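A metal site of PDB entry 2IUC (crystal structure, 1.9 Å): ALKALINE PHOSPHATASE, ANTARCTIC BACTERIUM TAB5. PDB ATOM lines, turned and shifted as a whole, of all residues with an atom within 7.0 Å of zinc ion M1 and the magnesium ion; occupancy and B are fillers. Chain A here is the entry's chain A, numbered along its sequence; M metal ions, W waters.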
ATOM      1  N   ILE A  41       6.021  25.675  -5.952  1.00  0.00           N
ATOM      2  CA  ILE A  41       5.454  26.517  -7.009  1.00  0.00           C
ATOM      3  C   ILE A  41       4.526  27.438  -6.300  1.00  0.00           C
ATOM      4  O   ILE A  41       3.596  26.980  -5.572  1.00  0.00           O
ATOM      5  CB  ILE A  41       4.651  25.636  -8.069  1.00  0.00           C
ATOM      6  CG1 ILE A  41       5.573  24.631  -8.756  1.00  0.00           C
ATOM      7  CG2 ILE A  41       3.810  26.575  -9.035  1.00  0.00           C
ATOM      8  CD1 ILE A  41       4.831  23.643  -9.701  1.00  0.00           C
ATOM      9  N   SER A  42       4.767  28.750  -6.444  1.00  0.00           N
ATOM     10  CA  SER A  42       3.884  29.755  -5.889  1.00  0.00           C
ATOM     11  C   SER A  42       3.029  30.171  -7.114  1.00  0.00           C
ATOM     12  O   SER A  42       3.500  30.880  -8.031  1.00  0.00           O
ATOM     13  CB  SER A  42       4.712  30.908  -5.389  1.00  0.00           C
ATOM     14  OG  SER A  42       5.755  31.154  -6.348  1.00  0.00           O
ATOM     15  N   ASP A  43       1.787  29.734  -7.113  1.00  0.00           N
ATOM     16  CA  ASP A  43       0.917  30.067  -8.212  1.00  0.00           C
ATOM     17  C   ASP A  43       0.618  31.522  -8.308  1.00  0.00           C
ATOM     18  O   ASP A  43       0.075  32.107  -7.363  1.00  0.00           O
ATOM     19  CB  ASP A  43      -0.403  29.310  -8.098  1.00  0.00           C
ATOM     20  CG  ASP A  43      -1.148  29.224  -9.469  1.00  0.00           C
ATOM     21  OD1 ASP A  43      -1.388  30.230 -10.095  1.00  0.00           O
ATOM     22  OD2 ASP A  43      -1.475  28.117  -9.922  1.00  0.00           O
ATOM     23  N   GLY A  44       0.954  32.130  -9.454  1.00  0.00           N
ATOM     24  CA  GLY A  44       0.613  33.534  -9.647  1.00  0.00           C
ATOM     25  C   GLY A  44       1.518  34.577  -9.022  1.00  0.00           C
ATOM     26  O   GLY A  44       1.141  35.728  -8.979  1.00  0.00           O
ATOM     27  N   THR A  82      -0.094  32.651 -20.256  1.00  0.00           N
ATOM     28  CA  THR A  82      -0.357  31.272 -19.953  1.00  0.00           C
ATOM     29  C   THR A  82      -1.450  31.181 -18.874  1.00  0.00           C
ATOM     30  O   THR A  82      -1.690  32.151 -18.160  1.00  0.00           O
ATOM     31  CB  THR A  82       0.936  30.595 -19.387  1.00  0.00           C
ATOM     32  OG1 THR A  82       0.717  29.175 -19.327  1.00  0.00           O
ATOM     33  CG2 THR A  82       1.186  31.088 -17.977  1.00  0.00           C
ATOM     34  N   ASP A  83      -2.079  30.036 -18.758  1.00  0.00           N
ATOM     35  CA  ASP A  83      -2.846  29.720 -17.520  1.00  0.00           C
ATOM     36  C   ASP A  83      -2.039  28.725 -16.683  1.00  0.00           C
ATOM     37  O   ASP A  83      -0.936  28.295 -17.074  1.00  0.00           O
ATOM     38  CB  ASP A  83      -4.297  29.208 -17.868  1.00  0.00           C
ATOM     39  CG  ASP A  83      -4.358  27.722 -18.246  1.00  0.00           C
ATOM     40  OD1 ASP A  83      -3.394  27.096 -18.795  1.00  0.00           O
ATOM     41  OD2 ASP A  83      -5.434  27.142 -18.026  1.00  0.00           O
ATOM     42  N   SER A  84      -2.603  28.303 -15.562  1.00  0.00           N
ATOM     43  CA  SER A  84      -1.849  27.395 -14.676  1.00  0.00           C
ATOM     44  C   SER A  84      -1.643  26.007 -15.260  1.00  0.00           C
ATOM     45  O   SER A  84      -0.706  25.247 -14.878  1.00  0.00           O
ATOM     46  CB  SER A  84      -2.709  27.170 -13.454  1.00  0.00           C
ATOM     47  OG  SER A  84      -2.778  28.392 -12.796  1.00  0.00           O
ATOM     48  N   ALA A  85      -2.597  25.601 -16.120  1.00  0.00           N
ATOM     49  CA  ALA A  85      -2.573  24.242 -16.679  1.00  0.00           C
ATOM     50  C   ALA A  85      -1.361  24.073 -17.610  1.00  0.00           C
ATOM     51  O   ALA A  85      -0.563  23.092 -17.413  1.00  0.00           O
ATOM     52  CB  ALA A  85      -3.836  23.948 -17.408  1.00  0.00           C
ATOM     53  N   GLY A  87       1.144  26.111 -17.866  1.00  0.00           N
ATOM     54  CA  GLY A  87       2.245  26.556 -16.997  1.00  0.00           C
ATOM     55  C   GLY A  87       2.834  25.403 -16.209  1.00  0.00           C
ATOM     56  O   GLY A  87       4.008  25.260 -16.184  1.00  0.00           O
ATOM     57  N   ALA A  88       2.002  24.613 -15.540  1.00  0.00           N
ATOM     58  CA  ALA A  88       2.509  23.547 -14.749  1.00  0.00           C
ATOM     59  C   ALA A  88       2.925  22.349 -15.628  1.00  0.00           C
ATOM     60  O   ALA A  88       3.777  21.567 -15.197  1.00  0.00           O
ATOM     61  CB  ALA A  88       1.478  23.078 -13.798  1.00  0.00           C
ATOM     62  N   SER A 131      -4.990  24.330  -2.758  1.00  0.00           N
ATOM     63  CA  SER A 131      -6.244  24.234  -3.517  1.00  0.00           C
ATOM     64  C   SER A 131      -6.766  22.813  -3.386  1.00  0.00           C
ATOM     65  O   SER A 131      -6.193  21.963  -2.631  1.00  0.00           O
ATOM     66  CB  SER A 131      -5.949  24.547  -4.997  1.00  0.00           C
ATOM     67  OG  SER A 131      -5.028  23.575  -5.473  1.00  0.00           O
ATOM     68  N   HIS A 135      -6.885  20.542  -8.698  1.00  0.00           N
ATOM     69  CA  HIS A 135      -6.671  21.867  -9.361  1.00  0.00           C
ATOM     70  C   HIS A 135      -5.488  21.776 -10.375  1.00  0.00           C
ATOM     71  O   HIS A 135      -4.749  20.834 -10.313  1.00  0.00           O
ATOM     72  CB  HIS A 135      -6.427  23.010  -8.337  1.00  0.00           C
ATOM     73  CG  HIS A 135      -6.968  24.336  -8.801  1.00  0.00           C
ATOM     74  ND1 HIS A 135      -6.157  25.326  -9.325  1.00  0.00           N
ATOM     75  CD2 HIS A 135      -8.250  24.819  -8.858  1.00  0.00           C
ATOM     76  CE1 HIS A 135      -6.921  26.354  -9.688  1.00  0.00           C
ATOM     77  NE2 HIS A 135      -8.190  26.073  -9.404  1.00  0.00           N
ATOM     78  N   ALA A 136      -5.369  22.716 -11.299  1.00  0.00           N
ATOM     79  CA  ALA A 136      -4.556  22.501 -12.487  1.00  0.00           C
ATOM     80  C   ALA A 136      -3.068  22.208 -12.154  1.00  0.00           C
ATOM     81  O   ALA A 136      -2.372  21.452 -12.832  1.00  0.00           O
ATOM     82  CB  ALA A 136      -4.674  23.696 -13.311  1.00  0.00           C
ATOM     83  N   THR A 137      -2.561  22.851 -11.122  1.00  0.00           N
ATOM     84  CA  THR A 137      -1.089  22.729 -10.826  1.00  0.00           C
ATOM     85  C   THR A 137      -0.748  21.333 -10.339  1.00  0.00           C
ATOM     86  O   THR A 137       0.042  20.647 -10.991  1.00  0.00           O
ATOM     87  CB  THR A 137      -0.599  23.884  -9.912  1.00  0.00           C
ATOM     88  OG1 THR A 137      -0.968  25.154 -10.484  1.00  0.00           O
ATOM     89  CG2 THR A 137       0.917  23.821  -9.627  1.00  0.00           C
ATOM     90  N   PRO A 138      -1.370  20.876  -9.176  1.00  0.00           N
ATOM     91  CA  PRO A 138      -1.076  19.480  -8.782  1.00  0.00           C
ATOM     92  C   PRO A 138      -1.446  18.445  -9.843  1.00  0.00           C
ATOM     93  O   PRO A 138      -0.760  17.397 -10.026  1.00  0.00           O
ATOM     94  CB  PRO A 138      -1.921  19.291  -7.483  1.00  0.00           C
ATOM     95  CG  PRO A 138      -2.906  20.431  -7.410  1.00  0.00           C
ATOM     96  CD  PRO A 138      -2.344  21.542  -8.274  1.00  0.00           C
ATOM     97  N   ARG A 148      -8.464  21.193 -18.066  1.00  0.00           N
ATOM     98  CA  ARG A 148      -8.282  21.268 -16.622  1.00  0.00           C
ATOM     99  C   ARG A 148      -9.603  21.266 -15.886  1.00  0.00           C
ATOM    100  O   ARG A 148      -9.598  21.043 -14.700  1.00  0.00           O
ATOM    101  CB  ARG A 148      -7.625  22.621 -16.264  1.00  0.00           C
ATOM    102  CG  ARG A 148      -8.453  23.859 -16.742  1.00  0.00           C
ATOM    103  CD  ARG A 148      -7.631  25.041 -16.463  1.00  0.00           C
ATOM    104  NE  ARG A 148      -7.527  25.294 -15.013  1.00  0.00           N
ATOM    105  CZ  ARG A 148      -6.896  26.341 -14.468  1.00  0.00           C
ATOM    106  NH1 ARG A 148      -6.219  27.210 -15.283  1.00  0.00           N
ATOM    107  NH2 ARG A 148      -6.904  26.510 -13.131  1.00  0.00           N
ATOM    108  N   GLU A 254       2.689  23.222  -3.594  1.00  0.00           N
ATOM    109  CA  GLU A 254       2.197  24.417  -4.261  1.00  0.00           C
ATOM    110  C   GLU A 254       1.536  25.356  -3.254  1.00  0.00           C
ATOM    111  O   GLU A 254       0.622  24.921  -2.487  1.00  0.00           O
ATOM    112  CB  GLU A 254       1.133  24.055  -5.325  1.00  0.00           C
ATOM    113  CG  GLU A 254       0.811  25.359  -6.105  1.00  0.00           C
ATOM    114  CD  GLU A 254      -0.551  25.310  -6.798  1.00  0.00           C
ATOM    115  OE1 GLU A 254      -1.374  24.438  -6.477  1.00  0.00           O
ATOM    116  OE2 GLU A 254      -0.761  26.136  -7.684  1.00  0.00           O
ATOM    117  N   GLY A 255       1.992  26.613  -3.243  1.00  0.00           N
ATOM    118  CA  GLY A 255       1.266  27.779  -2.620  1.00  0.00           C
ATOM    119  C   GLY A 255       0.165  28.251  -3.605  1.00  0.00           C
ATOM    120  O   GLY A 255       0.384  29.173  -4.413  1.00  0.00           O
ATOM    121  N   SER A 256      -0.961  27.531  -3.608  1.00  0.00           N
ATOM    122  CA  SER A 256      -2.047  27.652  -4.627  1.00  0.00           C
ATOM    123  C   SER A 256      -2.829  28.931  -4.616  1.00  0.00           C
ATOM    124  O   SER A 256      -3.323  29.385  -5.696  1.00  0.00           O
ATOM    125  CB  SER A 256      -3.066  26.500  -4.477  1.00  0.00           C
ATOM    126  OG  SER A 256      -2.402  25.290  -4.255  1.00  0.00           O
ATOM    127  N   GLN A 257      -2.994  29.526  -3.431  1.00  0.00           N
ATOM    128  CA  GLN A 257      -4.019  30.585  -3.286  1.00  0.00           C
ATOM    129  C   GLN A 257      -3.430  31.970  -3.473  1.00  0.00           C
ATOM    130  O   GLN A 257      -4.148  32.990  -3.523  1.00  0.00           O
ATOM    131  CB  GLN A 257      -4.743  30.449  -1.933  1.00  0.00           C
ATOM    132  CG  GLN A 257      -5.452  29.088  -1.888  1.00  0.00           C
ATOM    133  CD  GLN A 257      -6.430  29.033  -0.713  1.00  0.00           C
ATOM    134  OE1 GLN A 257      -6.998  30.041  -0.355  1.00  0.00           O
ATOM    135  NE2 GLN A 257      -6.667  27.832  -0.161  1.00  0.00           N
ATOM    136  N   ASP A 259      -2.390  33.098  -6.230  1.00  0.00           N
ATOM    137  CA  ASP A 259      -3.030  33.525  -7.500  1.00  0.00           C
ATOM    138  C   ASP A 259      -4.481  33.984  -7.237  1.00  0.00           C
ATOM    139  O   ASP A 259      -5.041  34.877  -7.891  1.00  0.00           O
ATOM    140  CB  ASP A 259      -3.026  32.286  -8.377  1.00  0.00           C
ATOM    141  CG  ASP A 259      -3.890  32.464  -9.638  1.00  0.00           C
ATOM    142  OD1 ASP A 259      -3.405  33.105 -10.579  1.00  0.00           O
ATOM    143  OD2 ASP A 259      -5.021  31.923  -9.671  1.00  0.00           O
ATOM    144  N   TRP A 260      -5.132  33.370  -6.261  1.00  0.00           N
ATOM    145  CA  TRP A 260      -6.566  33.719  -6.074  1.00  0.00           C
ATOM    146  C   TRP A 260      -6.691  35.078  -5.474  1.00  0.00           C
ATOM    147  O   TRP A 260      -7.634  35.792  -5.769  1.00  0.00           O
ATOM    148  CB  TRP A 260      -7.314  32.649  -5.248  1.00  0.00           C
ATOM    149  CG  TRP A 260      -7.204  31.207  -5.831  1.00  0.00           C
ATOM    150  CD1 TRP A 260      -6.659  30.827  -7.067  1.00  0.00           C
ATOM    151  CD2 TRP A 260      -7.667  30.002  -5.216  1.00  0.00           C
ATOM    152  NE1 TRP A 260      -6.766  29.468  -7.228  1.00  0.00           N
ATOM    153  CE2 TRP A 260      -7.400  28.929  -6.109  1.00  0.00           C
ATOM    154  CE3 TRP A 260      -8.337  29.723  -4.003  1.00  0.00           C
ATOM    155  CZ2 TRP A 260      -7.726  27.606  -5.805  1.00  0.00           C
ATOM    156  CZ3 TRP A 260      -8.659  28.417  -3.682  1.00  0.00           C
ATOM    157  CH2 TRP A 260      -8.393  27.376  -4.584  1.00  0.00           C
ATOM    158  N   HIS A 263      -6.225  37.474  -8.481  1.00  0.00           N
ATOM    159  CA  HIS A 263      -7.464  37.567  -9.279  1.00  0.00           C
ATOM    160  C   HIS A 263      -8.486  38.399  -8.549  1.00  0.00           C
ATOM    161  O   HIS A 263      -9.247  39.092  -9.196  1.00  0.00           O
ATOM    162  CB  HIS A 263      -8.113  36.191  -9.512  1.00  0.00           C
ATOM    163  CG  HIS A 263      -7.470  35.379 -10.600  1.00  0.00           C
ATOM    164  ND1 HIS A 263      -7.345  35.829 -11.913  1.00  0.00           N
ATOM    165  CD2 HIS A 263      -6.970  34.117 -10.585  1.00  0.00           C
ATOM    166  CE1 HIS A 263      -6.769  34.888 -12.648  1.00  0.00           C
ATOM    167  NE2 HIS A 263      -6.545  33.835 -11.867  1.00  0.00           N
ATOM    168  N   ASP A 301       4.220  29.677 -11.807  1.00  0.00           N
ATOM    169  CA  ASP A 301       3.771  29.468 -13.184  1.00  0.00           C
ATOM    170  C   ASP A 301       3.616  30.726 -14.062  1.00  0.00           C
ATOM    171  O   ASP A 301       3.764  30.640 -15.292  1.00  0.00           O
ATOM    172  CB  ASP A 301       2.502  28.604 -13.232  1.00  0.00           C
ATOM    173  CG  ASP A 301       1.344  29.140 -12.328  1.00  0.00           C
ATOM    174  OD1 ASP A 301       1.456  30.150 -11.583  1.00  0.00           O
ATOM    175  OD2 ASP A 301       0.219  28.610 -12.477  1.00  0.00           O
ATOM    176  N   HIS A 302       3.281  31.877 -13.464  1.00  0.00           N
ATOM    177  CA  HIS A 302       3.037  33.152 -14.169  1.00  0.00           C
ATOM    178  C   HIS A 302       2.689  34.111 -13.004  1.00  0.00           C
ATOM    179  O   HIS A 302       2.575  33.685 -11.828  1.00  0.00           O
ATOM    180  CB  HIS A 302       1.804  33.022 -15.150  1.00  0.00           C
ATOM    181  CG  HIS A 302       0.572  32.545 -14.413  1.00  0.00           C
ATOM    182  ND1 HIS A 302      -0.131  33.362 -13.561  1.00  0.00           N
ATOM    183  CD2 HIS A 302       0.032  31.317 -14.270  1.00  0.00           C
ATOM    184  CE1 HIS A 302      -1.028  32.672 -12.912  1.00  0.00           C
ATOM    185  NE2 HIS A 302      -0.980  31.441 -13.341  1.00  0.00           N
ATOM    186  N   THR A 304       0.025  37.131 -11.459  1.00  0.00           N
ATOM    187  CA  THR A 304      -1.402  37.537 -11.540  1.00  0.00           C
ATOM    188  C   THR A 304      -1.771  38.897 -10.902  1.00  0.00           C
ATOM    189  O   THR A 304      -1.389  39.221  -9.739  1.00  0.00           O
ATOM    190  CB  THR A 304      -2.287  36.525 -10.802  1.00  0.00           C
ATOM    191  OG1 THR A 304      -2.005  35.233 -11.271  1.00  0.00           O
ATOM    192  CG2 THR A 304      -3.867  36.842 -11.061  1.00  0.00           C
ATOM    193  N   HIS A 337      -4.000  36.993 -15.502  1.00  0.00           N
ATOM    194  CA  HIS A 337      -2.562  36.627 -15.481  1.00  0.00           C
ATOM    195  C   HIS A 337      -1.806  37.663 -16.294  1.00  0.00           C
ATOM    196  O   HIS A 337      -2.408  38.462 -17.038  1.00  0.00           O
ATOM    197  CB  HIS A 337      -2.391  35.216 -16.092  1.00  0.00           C
ATOM    198  CG  HIS A 337      -3.044  34.123 -15.288  1.00  0.00           C
ATOM    199  ND1 HIS A 337      -3.110  32.822 -15.732  1.00  0.00           N
ATOM    200  CD2 HIS A 337      -3.727  34.155 -14.094  1.00  0.00           C
ATOM    201  CE1 HIS A 337      -3.789  32.082 -14.840  1.00  0.00           C
ATOM    202  NE2 HIS A 337      -4.101  32.860 -13.820  1.00  0.00           N
HETATM  203 ZN    ZN M   1      -1.485  29.781 -12.103  1.00  0.00          ZN
HETATM  204 MG    MG M   2      -2.366  26.440  -9.113  1.00  0.00          MG
HETATM  205 ZN    ZN M   3      -5.034  32.361 -12.059  1.00  0.00          ZN
HETATM  206  O   HOH W   1      -3.876  26.349 -10.709  1.00  0.00           O
HETATM  207  O   HOH W   2      -3.543  24.779  -8.218  1.00  0.00           O
HETATM  208  O   HOH W   3      -3.486  27.833  -8.000  1.00  0.00           O
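N of Asp 43 sits at hydrogen-bond distance from O of Gly 255 (3.1 Å).
A ring nitrogen (NE2) of His 302 sits close to a ring nitrogen (ND1) of His 337 (3.5 Å).
OD1 of Asp 301 sits at hydrogen-bond distance from N of Gly 44 (3.0 Å).
The backbone carbonyl oxygen (O) of His 302 lies close to the backbone NH (N) of Gly 44 (3.3 Å).
OG of Ser 256 is in hydrogen-bond range of OE1 of Glu 254 (2.6 Å).
The backbone carbonyl oxygen of Asp 43 lies within hydrogen-bond range of the backbone NH of Asp 259.
Within 4 Å of zinc ion M1: Asp 43, Ser 84, Asp 301 and His 302.
Along chain A the residues within 4 Å of zinc ion M1 span positions 43 to 302.
The nearest printed residue that does not touch zinc ion M1 is Asp 259 (4.1 Å).
Residues that only touch the magnesium ion: His 135.
The nearest printed residue that does not touch the magnesium ion is Ser 84 (4.2 Å).
Zinc ion M1 is bound by OG of Ser 84 (2.0 Å), OD1 of Asp 43 (2.1 Å), OD2 of Asp 301 (2.1 Å) and NE2 of His 302 (2.1 Å).
Slightly farther from zinc ion M1 lies OD2 of Asp 43 (2.7 Å).
The magnesium ion is bound by the side-chain carboxylate of Asp 43 (2.1 Å), water W3 (2.1 Å), the side-chain carboxylate of Glu 254 (2.2 Å), water W1 (2.2 Å), water W2 (2.2 Å) and the side-chain hydroxyl of Thr 137 (2.3 Å).
The magnesium ion has six donor atoms within binding distance.
Water W2 lies within hydrogen-bond range of OE1 of Glu 254 (2.8 Å), ND1 of His 135 (2.9 Å) and OG of Ser 131 (3.3 Å).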
